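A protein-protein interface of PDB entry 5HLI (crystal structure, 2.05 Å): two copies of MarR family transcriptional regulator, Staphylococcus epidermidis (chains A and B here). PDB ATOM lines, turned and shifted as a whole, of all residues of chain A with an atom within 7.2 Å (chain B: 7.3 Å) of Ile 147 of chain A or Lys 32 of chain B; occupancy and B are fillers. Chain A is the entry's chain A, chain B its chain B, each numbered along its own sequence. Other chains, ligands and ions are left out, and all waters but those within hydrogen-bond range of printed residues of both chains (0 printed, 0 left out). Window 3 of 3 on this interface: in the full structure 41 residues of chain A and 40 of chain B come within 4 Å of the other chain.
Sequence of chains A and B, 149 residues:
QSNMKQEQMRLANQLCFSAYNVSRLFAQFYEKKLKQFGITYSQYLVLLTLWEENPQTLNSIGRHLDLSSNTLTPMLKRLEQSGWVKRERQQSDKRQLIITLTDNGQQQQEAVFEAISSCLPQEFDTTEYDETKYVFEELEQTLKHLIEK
The backbone carbonyl oxygen of Arg 24 of chain B sits at hydrogen-bond distance from the side-chain amide nitrogen of Gln 28 of chain B (3.1 Å).
No position is printed for both chains. Of the 8 pairs that touch across the chains among the printed residues, none has its exchanged pair printed and touching as well.
Printed residues of chain B within 4 Å of Ile 147 of chain A: Leu 25 (3.2 Å), Gln 28 (3.7 Å), Phe 29 (3.99 Å) and Lys 32 (3.9 Å). Of the printed residues of chain A, Lys 32 of chain B touches Ile 147. Printed residues of chain A within 4 Å of Phe 29 of chain B: Leu 143 (3.9 Å), Leu 146 (3.6 Å) and Ile 147 (3.99 Å). Printed residues of chain B within 4 Å of Leu 146 of chain A: Phe 29. Printed residues of chain A within 4 Å of Phe 26 of chain B: Leu 143 (3.8 Å). Of the printed residues of chain A, Leu 25 of chain B touches Leu 143 and Ile 147. Of the printed residues of chain A, Gln 28 of chain B touches Ile 147. Gln 36 of chain B touches none of the printed residues of chain A. Glu 148 of chain A touches none of the printed residues of chain B. The nearest printed residue of chain B that does not touch Ile 147 of chain A is Phe 26 of chain B (5.3 Å). The nearest printed residue of chain A that does not touch Lys 32 of chain B is Lys 149 of chain A (4.4 Å). The nearest printed residue of chain A that does not touch Phe 29 of chain B is Thr 142 of chain A (6.4 Å).
Printed residues of chain A that touch a printed residue of chain B: Leu 143, Leu 146 and Ile 147. Hydrophobic or aromatic side chains of chain A within 4 Å of the printed part of chain B: Leu 143, Leu 146 and Ile 147.
Among the printed residues, pairs that only touch across the chains: Ile 147 of chain A with Leu 25 of chain B, Leu 146 of chain A with Phe 29 of chain B, Ile 147 of chain A with Gln 28 of chain B, Leu 143 of chain A with Phe 26 of chain B, Leu 143 of chain A with Leu 25 of chain B, Ile 147 of chain A with Lys 32 of chain B, Leu 143 of chain A with Phe 29 of chain B and Ile 147 of chain A with Phe 29 of chain B.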
ATOM      1  N   THR A 142     -13.325  17.872  -8.229  1.00  0.00           N
ATOM      2  CA  THR A 142     -14.298  18.607  -9.033  1.00  0.00           C
ATOM      3  C   THR A 142     -15.639  18.718  -8.315  1.00  0.00           C
ATOM      4  O   THR A 142     -16.211  19.809  -8.221  1.00  0.00           O
ATOM      5  CB  THR A 142     -14.476  17.932 -10.395  1.00  0.00           C
ATOM      6  OG1 THR A 142     -13.237  17.969 -11.116  1.00  0.00           O
ATOM      7  CG2 THR A 142     -15.549  18.642 -11.210  1.00  0.00           C
ATOM      8  N   LEU A 143     -16.154  17.597  -7.803  1.00  0.00           N
ATOM      9  CA  LEU A 143     -17.466  17.616  -7.160  1.00  0.00           C
ATOM     10  C   LEU A 143     -17.466  18.521  -5.934  1.00  0.00           C
ATOM     11  O   LEU A 143     -18.439  19.244  -5.689  1.00  0.00           O
ATOM     12  CB  LEU A 143     -17.891  16.198  -6.788  1.00  0.00           C
ATOM     13  CG  LEU A 143     -18.087  15.250  -7.972  1.00  0.00           C
ATOM     14  CD1 LEU A 143     -18.361  13.832  -7.493  1.00  0.00           C
ATOM     15  CD2 LEU A 143     -19.204  15.742  -8.883  1.00  0.00           C
ATOM     16  N   LYS A 144     -16.381  18.499  -5.156  1.00  0.00           N
ATOM     17  CA  LYS A 144     -16.267  19.401  -4.014  1.00  0.00           C
ATOM     18  C   LYS A 144     -16.387  20.856  -4.450  1.00  0.00           C
ATOM     19  O   LYS A 144     -17.153  21.630  -3.866  1.00  0.00           O
ATOM     20  CB  LYS A 144     -14.941  19.161  -3.291  1.00  0.00           C
ATOM     21  CG  LYS A 144     -14.562  20.255  -2.304  1.00  0.00           C
ATOM     22  CD  LYS A 144     -13.174  20.016  -1.727  1.00  0.00           C
ATOM     23  CE  LYS A 144     -12.686  21.217  -0.929  1.00  0.00           C
ATOM     24  NZ  LYS A 144     -13.602  21.555   0.197  1.00  0.00           N
ATOM     25  N   HIS A 145     -15.644  21.242  -5.491  1.00  0.00           N
ATOM     26  CA  HIS A 145     -15.672  22.626  -5.956  1.00  0.00           C
ATOM     27  C   HIS A 145     -17.062  23.028  -6.441  1.00  0.00           C
ATOM     28  O   HIS A 145     -17.494  24.167  -6.235  1.00  0.00           O
ATOM     29  CB  HIS A 145     -14.639  22.819  -7.066  1.00  0.00           C
ATOM     30  CG  HIS A 145     -14.526  24.230  -7.551  1.00  0.00           C
ATOM     31  ND1 HIS A 145     -13.865  25.210  -6.842  1.00  0.00           N
ATOM     32  CD2 HIS A 145     -14.986  24.827  -8.676  1.00  0.00           C
ATOM     33  CE1 HIS A 145     -13.924  26.349  -7.508  1.00  0.00           C
ATOM     34  NE2 HIS A 145     -14.599  26.143  -8.624  1.00  0.00           N
ATOM     35  N   LEU A 146     -17.779  22.106  -7.089  1.00  0.00           N
ATOM     36  CA  LEU A 146     -19.105  22.431  -7.602  1.00  0.00           C
ATOM     37  C   LEU A 146     -20.135  22.494  -6.481  1.00  0.00           C
ATOM     38  O   LEU A 146     -21.046  23.330  -6.513  1.00  0.00           O
ATOM     39  CB  LEU A 146     -19.525  21.405  -8.652  1.00  0.00           C
ATOM     40  CG  LEU A 146     -18.632  21.336  -9.889  1.00  0.00           C
ATOM     41  CD1 LEU A 146     -19.065  20.181 -10.766  1.00  0.00           C
ATOM     42  CD2 LEU A 146     -18.675  22.648 -10.657  1.00  0.00           C
ATOM     43  N   ILE A 147     -20.009  21.613  -5.486  1.00  0.00           N
ATOM     44  CA  ILE A 147     -20.966  21.586  -4.384  1.00  0.00           C
ATOM     45  C   ILE A 147     -20.869  22.859  -3.552  1.00  0.00           C
ATOM     46  O   ILE A 147     -21.881  23.379  -3.066  1.00  0.00           O
ATOM     47  CB  ILE A 147     -20.740  20.324  -3.530  1.00  0.00           C
ATOM     48  CG1 ILE A 147     -21.231  19.084  -4.280  1.00  0.00           C
ATOM     49  CG2 ILE A 147     -21.428  20.448  -2.175  1.00  0.00           C
ATOM     50  CD1 ILE A 147     -20.797  17.780  -3.643  1.00  0.00           C
ATOM     51  N   GLU A 148     -19.659  23.391  -3.385  1.00  0.00           N
ATOM     52  CA  GLU A 148     -19.460  24.546  -2.521  1.00  0.00           C
ATOM     53  C   GLU A 148     -19.845  25.868  -3.180  1.00  0.00           C
ATOM     54  O   GLU A 148     -19.832  26.901  -2.504  1.00  0.00           O
ATOM     55  CB  GLU A 148     -18.004  24.592  -2.050  1.00  0.00           C
ATOM     56  CG  GLU A 148     -17.612  23.372  -1.220  1.00  0.00           C
ATOM     57  CD  GLU A 148     -16.379  23.602  -0.369  1.00  0.00           C
ATOM     58  OE1 GLU A 148     -15.269  23.683  -0.936  1.00  0.00           O
ATOM     59  OE2 GLU A 148     -16.519  23.702   0.869  1.00  0.00           O
ATOM     60  N   LYS A 149     -20.195  25.864  -4.462  1.00  0.00           N
ATOM     61  CA  LYS A 149     -20.685  27.075  -5.113  1.00  0.00           C
ATOM     62  C   LYS A 149     -22.030  27.490  -4.524  1.00  0.00           C
ATOM     63  O   LYS A 149     -22.879  26.644  -4.237  1.00  0.00           O
ATOM     64  CB  LYS A 149     -20.814  26.874  -6.625  1.00  0.00           C
ATOM     65  CG  LYS A 149     -19.491  26.788  -7.369  1.00  0.00           C
ATOM     66  CD  LYS A 149     -19.706  26.909  -8.872  1.00  0.00           C
ATOM     67  CE  LYS A 149     -18.408  26.711  -9.637  1.00  0.00           C
ATOM     68  NZ  LYS A 149     -17.307  27.553  -9.092  1.00  0.00           N
ATOM     69  OXT LYS A 149     -22.305  28.674  -4.322  1.00  0.00           O
ATOM     70  N   ARG B  24     -20.599   9.960  -1.700  1.00  0.00           N
ATOM     71  CA  ARG B  24     -21.268  11.023  -0.955  1.00  0.00           C
ATOM     72  C   ARG B  24     -21.324  12.314  -1.763  1.00  0.00           C
ATOM     73  O   ARG B  24     -22.334  13.027  -1.734  1.00  0.00           O
ATOM     74  CB  ARG B  24     -20.556  11.261   0.377  1.00  0.00           C
ATOM     75  CG  ARG B  24     -20.758  10.162   1.410  1.00  0.00           C
ATOM     76  CD  ARG B  24     -19.901  10.406   2.644  1.00  0.00           C
ATOM     77  NE  ARG B  24     -18.511  10.005   2.444  1.00  0.00           N
ATOM     78  CZ  ARG B  24     -18.056   8.770   2.645  1.00  0.00           C
ATOM     79  NH1 ARG B  24     -18.883   7.818   3.049  1.00  0.00           N
ATOM     80  NH2 ARG B  24     -16.776   8.485   2.441  1.00  0.00           N
ATOM     81  N   LEU B  25     -20.247  12.635  -2.481  1.00  0.00           N
ATOM     82  CA  LEU B  25     -20.196  13.893  -3.222  1.00  0.00           C
ATOM     83  C   LEU B  25     -21.151  13.880  -4.408  1.00  0.00           C
ATOM     84  O   LEU B  25     -21.757  14.907  -4.734  1.00  0.00           O
ATOM     85  CB  LEU B  25     -18.766  14.166  -3.684  1.00  0.00           C
ATOM     86  CG  LEU B  25     -17.743  14.375  -2.566  1.00  0.00           C
ATOM     87  CD1 LEU B  25     -16.327  14.382  -3.125  1.00  0.00           C
ATOM     88  CD2 LEU B  25     -18.036  15.666  -1.806  1.00  0.00           C
ATOM     89  N   PHE B  26     -21.297  12.718  -5.037  1.00  0.00           N
ATOM     90  CA  PHE B  26     -22.209  12.565  -6.162  1.00  0.00           C
ATOM     91  C   PHE B  26     -23.656  12.793  -5.731  1.00  0.00           C
ATOM     92  O   PHE B  26     -24.410  13.492  -6.407  1.00  0.00           O
ATOM     93  CB  PHE B  26     -22.060  11.176  -6.789  1.00  0.00           C
ATOM     94  CG  PHE B  26     -21.225  11.161  -8.036  1.00  0.00           C
ATOM     95  CD1 PHE B  26     -21.374  12.146  -8.998  1.00  0.00           C
ATOM     96  CD2 PHE B  26     -20.289  10.163  -8.246  1.00  0.00           C
ATOM     97  CE1 PHE B  26     -20.607  12.135 -10.148  1.00  0.00           C
ATOM     98  CE2 PHE B  26     -19.517  10.145  -9.394  1.00  0.00           C
ATOM     99  CZ  PHE B  26     -19.677  11.133 -10.346  1.00  0.00           C
ATOM    100  N   ALA B  27     -24.035  12.200  -4.604  1.00  0.00           N
ATOM    101  CA  ALA B  27     -25.391  12.348  -4.083  1.00  0.00           C
ATOM    102  C   ALA B  27     -25.729  13.811  -3.828  1.00  0.00           C
ATOM    103  O   ALA B  27     -26.825  14.271  -4.168  1.00  0.00           O
ATOM    104  CB  ALA B  27     -25.557  11.525  -2.805  1.00  0.00           C
ATOM    105  N   GLN B  28     -24.792  14.566  -3.248  1.00  0.00           N
ATOM    106  CA  GLN B  28     -25.024  15.989  -3.027  1.00  0.00           C
ATOM    107  C   GLN B  28     -25.048  16.753  -4.344  1.00  0.00           C
ATOM    108  O   GLN B  28     -25.863  17.664  -4.523  1.00  0.00           O
ATOM    109  CB  GLN B  28     -23.950  16.562  -2.104  1.00  0.00           C
ATOM    110  CG  GLN B  28     -23.738  15.771  -0.825  1.00  0.00           C
ATOM    111  CD  GLN B  28     -22.498  16.217  -0.070  1.00  0.00           C
ATOM    112  OE1 GLN B  28     -22.249  17.412   0.085  1.00  0.00           O
ATOM    113  NE2 GLN B  28     -21.717  15.255   0.404  1.00  0.00           N
ATOM    114  N   PHE B  29     -24.159  16.395  -5.275  1.00  0.00           N
ATOM    115  CA  PHE B  29     -24.101  17.079  -6.563  1.00  0.00           C
ATOM    116  C   PHE B  29     -25.409  16.920  -7.329  1.00  0.00           C
ATOM    117  O   PHE B  29     -25.984  17.904  -7.809  1.00  0.00           O
ATOM    118  CB  PHE B  29     -22.922  16.544  -7.380  1.00  0.00           C
ATOM    119  CG  PHE B  29     -22.878  17.053  -8.797  1.00  0.00           C
ATOM    120  CD1 PHE B  29     -22.378  18.312  -9.082  1.00  0.00           C
ATOM    121  CD2 PHE B  29     -23.327  16.264  -9.844  1.00  0.00           C
ATOM    122  CE1 PHE B  29     -22.335  18.781 -10.384  1.00  0.00           C
ATOM    123  CE2 PHE B  29     -23.286  16.726 -11.149  1.00  0.00           C
ATOM    124  CZ  PHE B  29     -22.789  17.985 -11.418  1.00  0.00           C
ATOM    125  N   TYR B  30     -25.901  15.683  -7.448  1.00  0.00           N
ATOM    126  CA  TYR B  30     -27.127  15.449  -8.205  1.00  0.00           C
ATOM    127  C   TYR B  30     -28.336  16.068  -7.517  1.00  0.00           C
ATOM    128  O   TYR B  30     -29.244  16.570  -8.186  1.00  0.00           O
ATOM    129  CB  TYR B  30     -27.345  13.952  -8.423  1.00  0.00           C
ATOM    130  CG  TYR B  30     -26.465  13.358  -9.501  1.00  0.00           C
ATOM    131  CD1 TYR B  30     -26.560  13.792 -10.818  1.00  0.00           C
ATOM    132  CD2 TYR B  30     -25.548  12.357  -9.205  1.00  0.00           C
ATOM    133  CE1 TYR B  30     -25.758  13.253 -11.808  1.00  0.00           C
ATOM    134  CE2 TYR B  30     -24.744  11.810 -10.189  1.00  0.00           C
ATOM    135  CZ  TYR B  30     -24.853  12.260 -11.489  1.00  0.00           C
ATOM    136  OH  TYR B  30     -24.055  11.717 -12.468  1.00  0.00           O
ATOM    137  N   GLU B  31     -28.372  16.036  -6.183  1.00  0.00           N
ATOM    138  CA  GLU B  31     -29.468  16.684  -5.470  1.00  0.00           C
ATOM    139  C   GLU B  31     -29.480  18.186  -5.736  1.00  0.00           C
ATOM    140  O   GLU B  31     -30.544  18.781  -5.936  1.00  0.00           O
ATOM    141  CB  GLU B  31     -29.363  16.403  -3.971  1.00  0.00           C
ATOM    142  CG  GLU B  31     -30.276  17.269  -3.110  1.00  0.00           C
ATOM    143  CD  GLU B  31     -30.104  17.015  -1.622  1.00  0.00           C
ATOM    144  OE1 GLU B  31     -29.614  15.927  -1.252  1.00  0.00           O
ATOM    145  OE2 GLU B  31     -30.456  17.905  -0.820  1.00  0.00           O
ATOM    146  N   LYS B  32     -28.298  18.806  -5.776  1.00  0.00           N
ATOM    147  CA  LYS B  32     -28.237  20.251  -5.976  1.00  0.00           C
ATOM    148  C   LYS B  32     -28.559  20.634  -7.414  1.00  0.00           C
ATOM    149  O   LYS B  32     -29.318  21.583  -7.651  1.00  0.00           O
ATOM    150  CB  LYS B  32     -26.860  20.779  -5.571  1.00  0.00           C
ATOM    151  CG  LYS B  32     -26.661  22.259  -5.864  1.00  0.00           C
ATOM    152  CD  LYS B  32     -25.782  22.930  -4.819  1.00  0.00           C
ATOM    153  CE  LYS B  32     -26.477  22.982  -3.466  1.00  0.00           C
ATOM    154  NZ  LYS B  32     -25.702  23.777  -2.476  1.00  0.00           N
ATOM    155  N   LYS B  33     -28.010  19.910  -8.394  1.00  0.00           N
ATOM    156  CA  LYS B  33     -28.204  20.280  -9.790  1.00  0.00           C
ATOM    157  C   LYS B  33     -29.557  19.858 -10.352  1.00  0.00           C
ATOM    158  O   LYS B  33     -30.026  20.476 -11.315  1.00  0.00           O
ATOM    159  CB  LYS B  33     -27.084  19.695 -10.655  1.00  0.00           C
ATOM    160  CG  LYS B  33     -25.682  20.169 -10.278  1.00  0.00           C
ATOM    161  CD  LYS B  33     -25.599  21.690 -10.160  1.00  0.00           C
ATOM    162  CE  LYS B  33     -25.891  22.395 -11.484  1.00  0.00           C
ATOM    163  NZ  LYS B  33     -24.739  22.349 -12.428  1.00  0.00           N
ATOM    164  N   LEU B  34     -30.193  18.830  -9.791  1.00  0.00           N
ATOM    165  CA  LEU B  34     -31.492  18.389 -10.283  1.00  0.00           C
ATOM    166  C   LEU B  34     -32.661  19.099  -9.614  1.00  0.00           C
ATOM    167  O   LEU B  34     -33.800  18.937 -10.067  1.00  0.00           O
ATOM    168  CB  LEU B  34     -31.652  16.877 -10.099  1.00  0.00           C
ATOM    169  CG  LEU B  34     -30.710  15.982 -10.907  1.00  0.00           C
ATOM    170  CD1 LEU B  34     -30.966  14.515 -10.588  1.00  0.00           C
ATOM    171  CD2 LEU B  34     -30.857  16.246 -12.397  1.00  0.00           C
ATOM    172  N   LYS B  35     -32.405  19.880  -8.557  1.00  0.00           N
ATOM    173  CA  LYS B  35     -33.480  20.569  -7.847  1.00  0.00           C
ATOM    174  C   LYS B  35     -34.295  21.453  -8.782  1.00  0.00           C
ATOM    175  O   LYS B  35     -35.524  21.519  -8.672  1.00  0.00           O
ATOM    176  CB  LYS B  35     -32.898  21.410  -6.709  1.00  0.00           C
ATOM    177  CG  LYS B  35     -33.936  21.968  -5.743  1.00  0.00           C
ATOM    178  CD  LYS B  35     -34.399  20.898  -4.763  1.00  0.00           C
ATOM    179  CE  LYS B  35     -35.426  21.435  -3.779  1.00  0.00           C
ATOM    180  NZ  LYS B  35     -36.745  21.675  -4.422  1.00  0.00           N
ATOM    181  N   GLN B  36     -33.624  22.142  -9.708  1.00  0.00           N
ATOM    182  CA  GLN B  36     -34.309  23.053 -10.620  1.00  0.00           C
ATOM    183  C   GLN B  36     -35.331  22.343 -11.499  1.00  0.00           C
ATOM    184  O   GLN B  36     -36.243  22.995 -12.019  1.00  0.00           O
ATOM    185  CB  GLN B  36     -33.286  23.771 -11.499  1.00  0.00           C
ATOM    186  CG  GLN B  36     -32.421  22.824 -12.310  1.00  0.00           C
ATOM    187  CD  GLN B  36     -31.335  23.537 -13.083  1.00  0.00           C
ATOM    188  OE1 GLN B  36     -31.590  24.529 -13.767  1.00  0.00           O
ATOM    189  NE2 GLN B  36     -30.109  23.036 -12.976  1.00  0.00           N
ATOM    190  N   PHE B  37     -35.199  21.029 -11.683  1.00  0.00           N
ATOM    191  CA  PHE B  37     -36.128  20.260 -12.498  1.00  0.00           C
ATOM    192  C   PHE B  37     -37.158  19.500 -11.675  1.00  0.00           C
ATOM    193  O   PHE B  37     -38.081  18.920 -12.254  1.00  0.00           O
ATOM    194  CB  PHE B  37     -35.360  19.274 -13.388  1.00  0.00           C
ATOM    195  CG  PHE B  37     -34.273  19.915 -14.199  1.00  0.00           C
ATOM    196  CD1 PHE B  37     -34.584  20.758 -15.256  1.00  0.00           C
ATOM    197  CD2 PHE B  37     -32.942  19.679 -13.905  1.00  0.00           C
ATOM    198  CE1 PHE B  37     -33.587  21.353 -16.003  1.00  0.00           C
ATOM    199  CE2 PHE B  37     -31.937  20.272 -14.652  1.00  0.00           C
ATOM    200  CZ  PHE B  37     -32.260  21.110 -15.701  1.00  0.00           C
ATOM    201  N   ILE B 116     -25.808  18.798 -15.565  1.00  0.00           N
ATOM    202  CA  ILE B 116     -25.097  17.669 -14.979  1.00  0.00           C
ATOM    203  C   ILE B 116     -23.670  17.546 -15.515  1.00  0.00           C
ATOM    204  O   ILE B 116     -22.786  17.056 -14.804  1.00  0.00           O
ATOM    205  CB  ILE B 116     -25.900  16.376 -15.226  1.00  0.00           C
ATOM    206  CG1 ILE B 116     -27.284  16.480 -14.581  1.00  0.00           C
ATOM    207  CG2 ILE B 116     -25.162  15.158 -14.700  1.00  0.00           C
ATOM    208  CD1 ILE B 116     -27.245  16.802 -13.106  1.00  0.00           C
